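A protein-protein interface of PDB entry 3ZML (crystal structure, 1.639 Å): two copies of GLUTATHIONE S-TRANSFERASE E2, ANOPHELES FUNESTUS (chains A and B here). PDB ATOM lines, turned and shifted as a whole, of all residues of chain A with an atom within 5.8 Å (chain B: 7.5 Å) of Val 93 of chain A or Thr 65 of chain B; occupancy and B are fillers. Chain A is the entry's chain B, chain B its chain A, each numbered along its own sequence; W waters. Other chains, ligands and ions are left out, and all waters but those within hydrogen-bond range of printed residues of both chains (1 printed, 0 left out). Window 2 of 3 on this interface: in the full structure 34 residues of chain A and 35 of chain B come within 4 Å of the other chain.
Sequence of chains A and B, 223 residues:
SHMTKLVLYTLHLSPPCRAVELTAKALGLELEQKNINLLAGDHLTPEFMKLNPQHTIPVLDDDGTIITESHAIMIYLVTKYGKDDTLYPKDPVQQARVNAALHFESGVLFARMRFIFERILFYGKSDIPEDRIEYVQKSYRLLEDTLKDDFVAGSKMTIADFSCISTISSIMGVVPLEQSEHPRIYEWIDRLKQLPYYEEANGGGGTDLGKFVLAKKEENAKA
Printed residues of chain B within 4 Å of Val 93 of chain A: Thr 65. Of the printed residues of chain B, Ala 96 of chain A touches Ile 67. Asp 63 of chain B touches none of the printed residues of chain A. Of the printed residues of chain A, Ile 67 of chain B touches Ala 96. Of the printed residues of chain A, Tyr 76 of chain B touches Pro 92 (3.9 Å). The nearest residue of chain B that does not touch Val 93 of chain A is Ile 67 of chain B (4.05 Å). The nearest printed residue of chain A that does not touch Thr 65 of chain B is Gln 94 of chain A (7.5 Å).
The backbone carbonyl oxygen (O) of Leu 60 of chain B is in hydrogen-bond range of the backbone NH (N) of Ile 67 of chain B (2.8 Å). OH of Tyr 76 of chain B sits at hydrogen-bond distance from OD2 of Asp 62 of chain B, 2.6 Å away. OD2 of Asp 91 of chain A is in hydrogen-bond range of N of Val 93 of chain A, at 3.2 Å.
Water W1 lies within hydrogen-bond range of OG1 of Thr 79 of chain B (2.9 Å) and NE2 of Gln 95 of chain A (3.0 Å).
O of Pro 92 of chain A touches CD1 of Tyr 76 of chain B, 3.9 Å away. CG1 of Val 93 of chain A touches CG2 of Thr 65 of chain B, 3.9 Å away. Ile 67 of chain B touches Ala 96 of chain A.
Hydrophobic or aromatic side chains of chain A within 4 Å of the printed part of chain B: Val 93 and Ala 96. Along chain A the printed residues that touch a printed residue of chain B span positions 92 to 96. Printed residues of chain B that touch a printed residue of chain A: Thr 65, Ile 67 and Tyr 76. Hydrophobic or aromatic side chains of chain B that line the printed part of chain A: Ile 67 and Tyr 76. Among the printed residues, 3 pairs touch across the chains. Among the printed residues, no Asp or Glu carboxylate lies within 4 Å of a Lys or Arg side-chain nitrogen of the other chain.
No position is printed for both chains. Of the 3 pairs that touch across the chains among the printed residues, none has its exchanged pair printed and touching as well.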
ATOM      1  N   ASP A  91      -8.157  33.582  36.399  1.00  0.00           N
ATOM      2  CA  ASP A  91      -8.706  32.467  35.607  1.00  0.00           C
ATOM      3  C   ASP A  91      -7.899  32.392  34.275  1.00  0.00           C
ATOM      4  O   ASP A  91      -7.823  33.415  33.584  1.00  0.00           O
ATOM      5  CB  ASP A  91     -10.171  32.678  35.248  1.00  0.00           C
ATOM      6  CG  ASP A  91     -10.669  31.596  34.323  1.00  0.00           C
ATOM      7  OD1 ASP A  91     -10.794  30.436  34.790  1.00  0.00           O
ATOM      8  OD2 ASP A  91     -10.886  31.801  33.112  1.00  0.00           O
ATOM      9  N   PRO A  92      -7.359  31.223  33.905  1.00  0.00           N
ATOM     10  CA  PRO A  92      -6.464  31.205  32.744  1.00  0.00           C
ATOM     11  C   PRO A  92      -7.106  31.625  31.418  1.00  0.00           C
ATOM     12  O   PRO A  92      -6.477  32.282  30.588  1.00  0.00           O
ATOM     13  CB  PRO A  92      -5.965  29.739  32.723  1.00  0.00           C
ATOM     14  CG  PRO A  92      -6.069  29.318  34.177  1.00  0.00           C
ATOM     15  CD  PRO A  92      -7.366  29.927  34.616  1.00  0.00           C
ATOM     16  N   VAL A  93      -8.376  31.278  31.197  1.00  0.00           N
ATOM     17  CA  VAL A  93      -9.076  31.662  29.984  1.00  0.00           C
ATOM     18  C   VAL A  93      -9.380  33.164  29.920  1.00  0.00           C
ATOM     19  O   VAL A  93      -9.057  33.806  28.942  1.00  0.00           O
ATOM     20  CB  VAL A  93     -10.350  30.821  29.797  1.00  0.00           C
ATOM     21  CG1 VAL A  93     -11.016  31.145  28.476  1.00  0.00           C
ATOM     22  CG2 VAL A  93      -9.966  29.350  29.812  1.00  0.00           C
ATOM     23  N   GLN A  94     -10.023  33.705  30.951  1.00  0.00           N
ATOM     24  CA  GLN A  94     -10.270  35.136  31.002  1.00  0.00           C
ATOM     25  C   GLN A  94      -8.944  35.919  30.985  1.00  0.00           C
ATOM     26  O   GLN A  94      -8.833  36.928  30.307  1.00  0.00           O
ATOM     27  CB  GLN A  94     -11.070  35.502  32.220  1.00  0.00           C
ATOM     28  CG  GLN A  94     -12.496  34.927  32.201  1.00  0.00           C
ATOM     29  CD  GLN A  94     -13.170  35.121  33.550  1.00  0.00           C
ATOM     30  OE1 GLN A  94     -12.832  36.026  34.282  1.00  0.00           O
ATOM     31  NE2 GLN A  94     -14.129  34.269  33.872  1.00  0.00           N
ATOM     32  N   GLN A  95      -7.926  35.443  31.672  1.00  0.00           N
ATOM     33  CA  GLN A  95      -6.608  36.119  31.602  1.00  0.00           C
ATOM     34  C   GLN A  95      -6.063  36.131  30.195  1.00  0.00           C
ATOM     35  O   GLN A  95      -5.451  37.121  29.793  1.00  0.00           O
ATOM     36  CB  GLN A  95      -5.582  35.417  32.510  1.00  0.00           C
ATOM     37  CG  GLN A  95      -4.418  36.321  32.782  1.00  0.00           C
ATOM     38  CD  GLN A  95      -3.365  35.742  33.703  1.00  0.00           C
ATOM     39  OE1 GLN A  95      -3.534  35.704  34.922  1.00  0.00           O
ATOM     40  NE2 GLN A  95      -2.264  35.331  33.130  1.00  0.00           N
ATOM     41  N   ALA A  96      -6.203  35.011  29.485  1.00  0.00           N
ATOM     42  CA  ALA A  96      -5.731  34.955  28.096  1.00  0.00           C
ATOM     43  C   ALA A  96      -6.414  35.974  27.214  1.00  0.00           C
ATOM     44  O   ALA A  96      -5.782  36.563  26.348  1.00  0.00           O
ATOM     45  CB  ALA A  96      -5.817  33.531  27.495  1.00  0.00           C
ATOM     46  N   ARG A  97      -7.697  36.236  27.465  1.00  0.00           N
ATOM     47  CA  ARG A  97      -8.434  37.213  26.675  1.00  0.00           C
ATOM     48  C   ARG A  97      -7.881  38.637  26.963  1.00  0.00           C
ATOM     49  O   ARG A  97      -7.745  39.471  26.022  1.00  0.00           O
ATOM     50  CB  ARG A  97      -9.949  37.045  26.950  1.00  0.00           C
ATOM     51  CG  ARG A  97     -10.786  38.061  26.171  1.00  0.00           C
ATOM     52  CD  ARG A  97     -12.281  37.794  26.311  1.00  0.00           C
ATOM     53  NE  ARG A  97     -13.019  38.681  25.412  1.00  0.00           N
ATOM     54  CZ  ARG A  97     -14.322  38.898  25.540  1.00  0.00           C
ATOM     55  NH1 ARG A  97     -15.005  38.284  26.519  1.00  0.00           N
ATOM     56  NH2 ARG A  97     -14.931  39.712  24.677  1.00  0.00           N
ATOM     57  N   VAL A  98      -7.522  38.882  28.220  1.00  0.00           N
ATOM     58  CA  VAL A  98      -6.943  40.149  28.586  1.00  0.00           C
ATOM     59  C   VAL A  98      -5.540  40.249  27.948  1.00  0.00           C
ATOM     60  O   VAL A  98      -5.180  41.281  27.365  1.00  0.00           O
ATOM     61  CB  VAL A  98      -6.865  40.324  30.129  1.00  0.00           C
ATOM     62  CG1 VAL A  98      -6.122  41.617  30.550  1.00  0.00           C
ATOM     63  CG2 VAL A  98      -8.287  40.321  30.706  1.00  0.00           C
ATOM     64  N   LEU B   6      -5.023  19.338  21.652  1.00  0.00           N
ATOM     65  CA  LEU B   6      -4.737  20.778  21.352  1.00  0.00           C
ATOM     66  C   LEU B   6      -4.587  21.046  19.849  1.00  0.00           C
ATOM     67  O   LEU B   6      -3.806  20.366  19.145  1.00  0.00           O
ATOM     68  CB  LEU B   6      -3.486  21.274  22.128  1.00  0.00           C
ATOM     69  CG  LEU B   6      -3.496  21.306  23.658  1.00  0.00           C
ATOM     70  CD1 LEU B   6      -2.022  21.493  24.096  1.00  0.00           C
ATOM     71  CD2 LEU B   6      -4.394  22.375  24.262  1.00  0.00           C
ATOM     72  N   VAL B   7      -5.335  22.012  19.325  1.00  0.00           N
ATOM     73  CA  VAL B   7      -5.328  22.303  17.874  1.00  0.00           C
ATOM     74  C   VAL B   7      -4.810  23.737  17.675  1.00  0.00           C
ATOM     75  O   VAL B   7      -5.221  24.641  18.399  1.00  0.00           O
ATOM     76  CB  VAL B   7      -6.762  22.233  17.279  1.00  0.00           C
ATOM     77  CG1 VAL B   7      -6.822  22.772  15.877  1.00  0.00           C
ATOM     78  CG2 VAL B   7      -7.308  20.801  17.253  1.00  0.00           C
ATOM     79  N   VAL B  59      -4.183  30.886  16.416  1.00  0.00           N
ATOM     80  CA  VAL B  59      -5.303  30.743  17.328  1.00  0.00           C
ATOM     81  C   VAL B  59      -5.275  29.290  17.841  1.00  0.00           C
ATOM     82  O   VAL B  59      -5.079  28.332  17.047  1.00  0.00           O
ATOM     83  CB  VAL B  59      -6.648  31.005  16.576  1.00  0.00           C
ATOM     84  CG1 VAL B  59      -7.834  30.739  17.514  1.00  0.00           C
ATOM     85  CG2 VAL B  59      -6.703  32.455  16.112  1.00  0.00           C
ATOM     86  N   LEU B  60      -5.436  29.108  19.153  1.00  0.00           N
ATOM     87  CA  LEU B  60      -5.492  27.790  19.775  1.00  0.00           C
ATOM     88  C   LEU B  60      -6.933  27.352  20.068  1.00  0.00           C
ATOM     89  O   LEU B  60      -7.733  28.135  20.621  1.00  0.00           O
ATOM     90  CB  LEU B  60      -4.760  27.831  21.104  1.00  0.00           C
ATOM     91  CG  LEU B  60      -4.645  26.542  21.951  1.00  0.00           C
ATOM     92  CD1 LEU B  60      -3.628  25.639  21.228  1.00  0.00           C
ATOM     93  CD2 LEU B  60      -4.300  26.764  23.428  1.00  0.00           C
ATOM     94  N   ASP B  61      -7.259  26.103  19.712  1.00  0.00           N
ATOM     95  CA  ASP B  61      -8.488  25.436  20.189  1.00  0.00           C
ATOM     96  C   ASP B  61      -8.068  24.344  21.193  1.00  0.00           C
ATOM     97  O   ASP B  61      -7.476  23.303  20.822  1.00  0.00           O
ATOM     98  CB  ASP B  61      -9.340  24.917  18.998  1.00  0.00           C
ATOM     99  CG  ASP B  61     -10.562  24.063  19.409  1.00  0.00           C
ATOM    100  OD1 ASP B  61     -10.665  23.600  20.572  1.00  0.00           O
ATOM    101  OD2 ASP B  61     -11.429  23.845  18.497  1.00  0.00           O
ATOM    102  N   ASP B  62      -8.347  24.620  22.455  1.00  0.00           N
ATOM    103  CA  ASP B  62      -8.082  23.660  23.540  1.00  0.00           C
ATOM    104  C   ASP B  62      -9.430  23.021  23.903  1.00  0.00           C
ATOM    105  O   ASP B  62     -10.163  23.562  24.719  1.00  0.00           O
ATOM    106  CB  ASP B  62      -7.466  24.366  24.766  1.00  0.00           C
ATOM    107  CG  ASP B  62      -7.077  23.389  25.894  1.00  0.00           C
ATOM    108  OD1 ASP B  62      -7.425  22.148  25.827  1.00  0.00           O
ATOM    109  OD2 ASP B  62      -6.347  23.815  26.814  1.00  0.00           O
ATOM    110  N   ASP B  63      -9.742  21.894  23.258  1.00  0.00           N
ATOM    111  CA  ASP B  63     -10.963  21.159  23.595  1.00  0.00           C
ATOM    112  C   ASP B  63     -12.213  22.055  23.514  1.00  0.00           C
ATOM    113  O   ASP B  63     -13.058  22.034  24.417  1.00  0.00           O
ATOM    114  CB  ASP B  63     -10.810  20.543  24.987  1.00  0.00           C
ATOM    115  CG  ASP B  63     -11.938  19.560  25.324  1.00  0.00           C
ATOM    116  OD1 ASP B  63     -12.459  18.899  24.399  1.00  0.00           O
ATOM    117  OD2 ASP B  63     -12.304  19.453  26.513  1.00  0.00           O
ATOM    118  N   GLY B  64     -12.305  22.847  22.436  1.00  0.00           N
ATOM    119  CA  GLY B  64     -13.416  23.796  22.220  1.00  0.00           C
ATOM    120  C   GLY B  64     -13.252  25.214  22.809  1.00  0.00           C
ATOM    121  O   GLY B  64     -13.985  26.130  22.457  1.00  0.00           O
ATOM    122  N   THR B  65     -12.270  25.415  23.661  1.00  0.00           N
ATOM    123  CA  THR B  65     -12.006  26.744  24.200  1.00  0.00           C
ATOM    124  C   THR B  65     -11.004  27.435  23.225  1.00  0.00           C
ATOM    125  O   THR B  65      -9.896  26.900  22.950  1.00  0.00           O
ATOM    126  CB  THR B  65     -11.446  26.658  25.611  1.00  0.00           C
ATOM    127  OG1 THR B  65     -12.455  26.085  26.478  1.00  0.00           O
ATOM    128  CG2 THR B  65     -11.147  28.032  26.148  1.00  0.00           C
ATOM    129  N   ILE B  66     -11.431  28.596  22.745  1.00  0.00           N
ATOM    130  CA  ILE B  66     -10.688  29.324  21.700  1.00  0.00           C
ATOM    131  C   ILE B  66      -9.825  30.415  22.356  1.00  0.00           C
ATOM    132  O   ILE B  66     -10.356  31.307  23.045  1.00  0.00           O
ATOM    133  CB  ILE B  66     -11.594  29.904  20.579  1.00  0.00           C
ATOM    134  CG1 ILE B  66     -12.528  28.796  20.035  1.00  0.00           C
ATOM    135  CG2 ILE B  66     -10.766  30.658  19.533  1.00  0.00           C
ATOM    136  CD1 ILE B  66     -11.819  27.598  19.425  1.00  0.00           C
ATOM    137  N   ILE B  67      -8.508  30.341  22.130  1.00  0.00           N
ATOM    138  CA  ILE B  67      -7.551  31.278  22.767  1.00  0.00           C
ATOM    139  C   ILE B  67      -6.780  31.928  21.609  1.00  0.00           C
ATOM    140  O   ILE B  67      -6.098  31.238  20.863  1.00  0.00           O
ATOM    141  CB  ILE B  67      -6.561  30.576  23.736  1.00  0.00           C
ATOM    142  CG1 ILE B  67      -7.262  29.699  24.832  1.00  0.00           C
ATOM    143  CG2 ILE B  67      -5.642  31.618  24.394  1.00  0.00           C
ATOM    144  CD1 ILE B  67      -8.096  30.533  25.741  1.00  0.00           C
ATOM    145  N   THR B  68      -6.933  33.242  21.442  1.00  0.00           N
ATOM    146  CA  THR B  68      -6.212  33.920  20.330  1.00  0.00           C
ATOM    147  C   THR B  68      -4.891  34.524  20.864  1.00  0.00           C
ATOM    148  O   THR B  68      -4.697  34.734  22.070  1.00  0.00           O
ATOM    149  CB  THR B  68      -7.027  35.066  19.711  1.00  0.00           C
ATOM    150  OG1 THR B  68      -7.129  36.116  20.694  1.00  0.00           O
ATOM    151  CG2 THR B  68      -8.447  34.626  19.269  1.00  0.00           C
ATOM    152  N   TYR B  76      -0.816  30.837  28.459  1.00  0.00           N
ATOM    153  CA  TYR B  76      -1.873  29.906  28.781  1.00  0.00           C
ATOM    154  C   TYR B  76      -1.346  28.486  28.809  1.00  0.00           C
ATOM    155  O   TYR B  76      -1.642  27.712  29.767  1.00  0.00           O
ATOM    156  CB  TYR B  76      -3.016  30.024  27.756  1.00  0.00           C
ATOM    157  CG  TYR B  76      -4.078  28.968  27.879  1.00  0.00           C
ATOM    158  CD1 TYR B  76      -5.128  29.085  28.788  1.00  0.00           C
ATOM    159  CD2 TYR B  76      -4.029  27.835  27.021  1.00  0.00           C
ATOM    160  CE1 TYR B  76      -6.146  28.121  28.843  1.00  0.00           C
ATOM    161  CE2 TYR B  76      -5.000  26.872  27.065  1.00  0.00           C
ATOM    162  CZ  TYR B  76      -6.050  27.002  27.986  1.00  0.00           C
ATOM    163  OH  TYR B  76      -7.026  26.023  28.092  1.00  0.00           O
ATOM    164  N   THR B  79       0.963  28.015  31.918  1.00  0.00           N
ATOM    165  CA  THR B  79       0.113  28.031  33.135  1.00  0.00           C
ATOM    166  C   THR B  79      -0.657  26.706  33.293  1.00  0.00           C
ATOM    167  O   THR B  79      -0.641  26.059  34.348  1.00  0.00           O
ATOM    168  CB  THR B  79      -0.928  29.179  33.059  1.00  0.00           C
ATOM    169  OG1 THR B  79      -0.230  30.420  32.924  1.00  0.00           O
ATOM    170  CG2 THR B  79      -1.930  29.140  34.320  1.00  0.00           C
ATOM    171  N   LYS B  80      -1.305  26.264  32.238  1.00  0.00           N
ATOM    172  CA  LYS B  80      -2.197  25.075  32.309  1.00  0.00           C
ATOM    173  C   LYS B  80      -1.422  23.741  32.284  1.00  0.00           C
ATOM    174  O   LYS B  80      -1.869  22.751  32.924  1.00  0.00           O
ATOM    175  CB  LYS B  80      -3.228  25.137  31.189  1.00  0.00           C
ATOM    176  CG  LYS B  80      -4.417  24.188  31.421  1.00  0.00           C
ATOM    177  CD  LYS B  80      -5.590  24.599  30.543  1.00  0.00           C
ATOM    178  CE  LYS B  80      -6.477  23.416  30.148  1.00  0.00           C
ATOM    179  NZ  LYS B  80      -7.292  23.011  31.308  1.00  0.00           N
HETATM  180  O   HOH W   1      -2.423  32.328  33.160  1.00  0.00           O
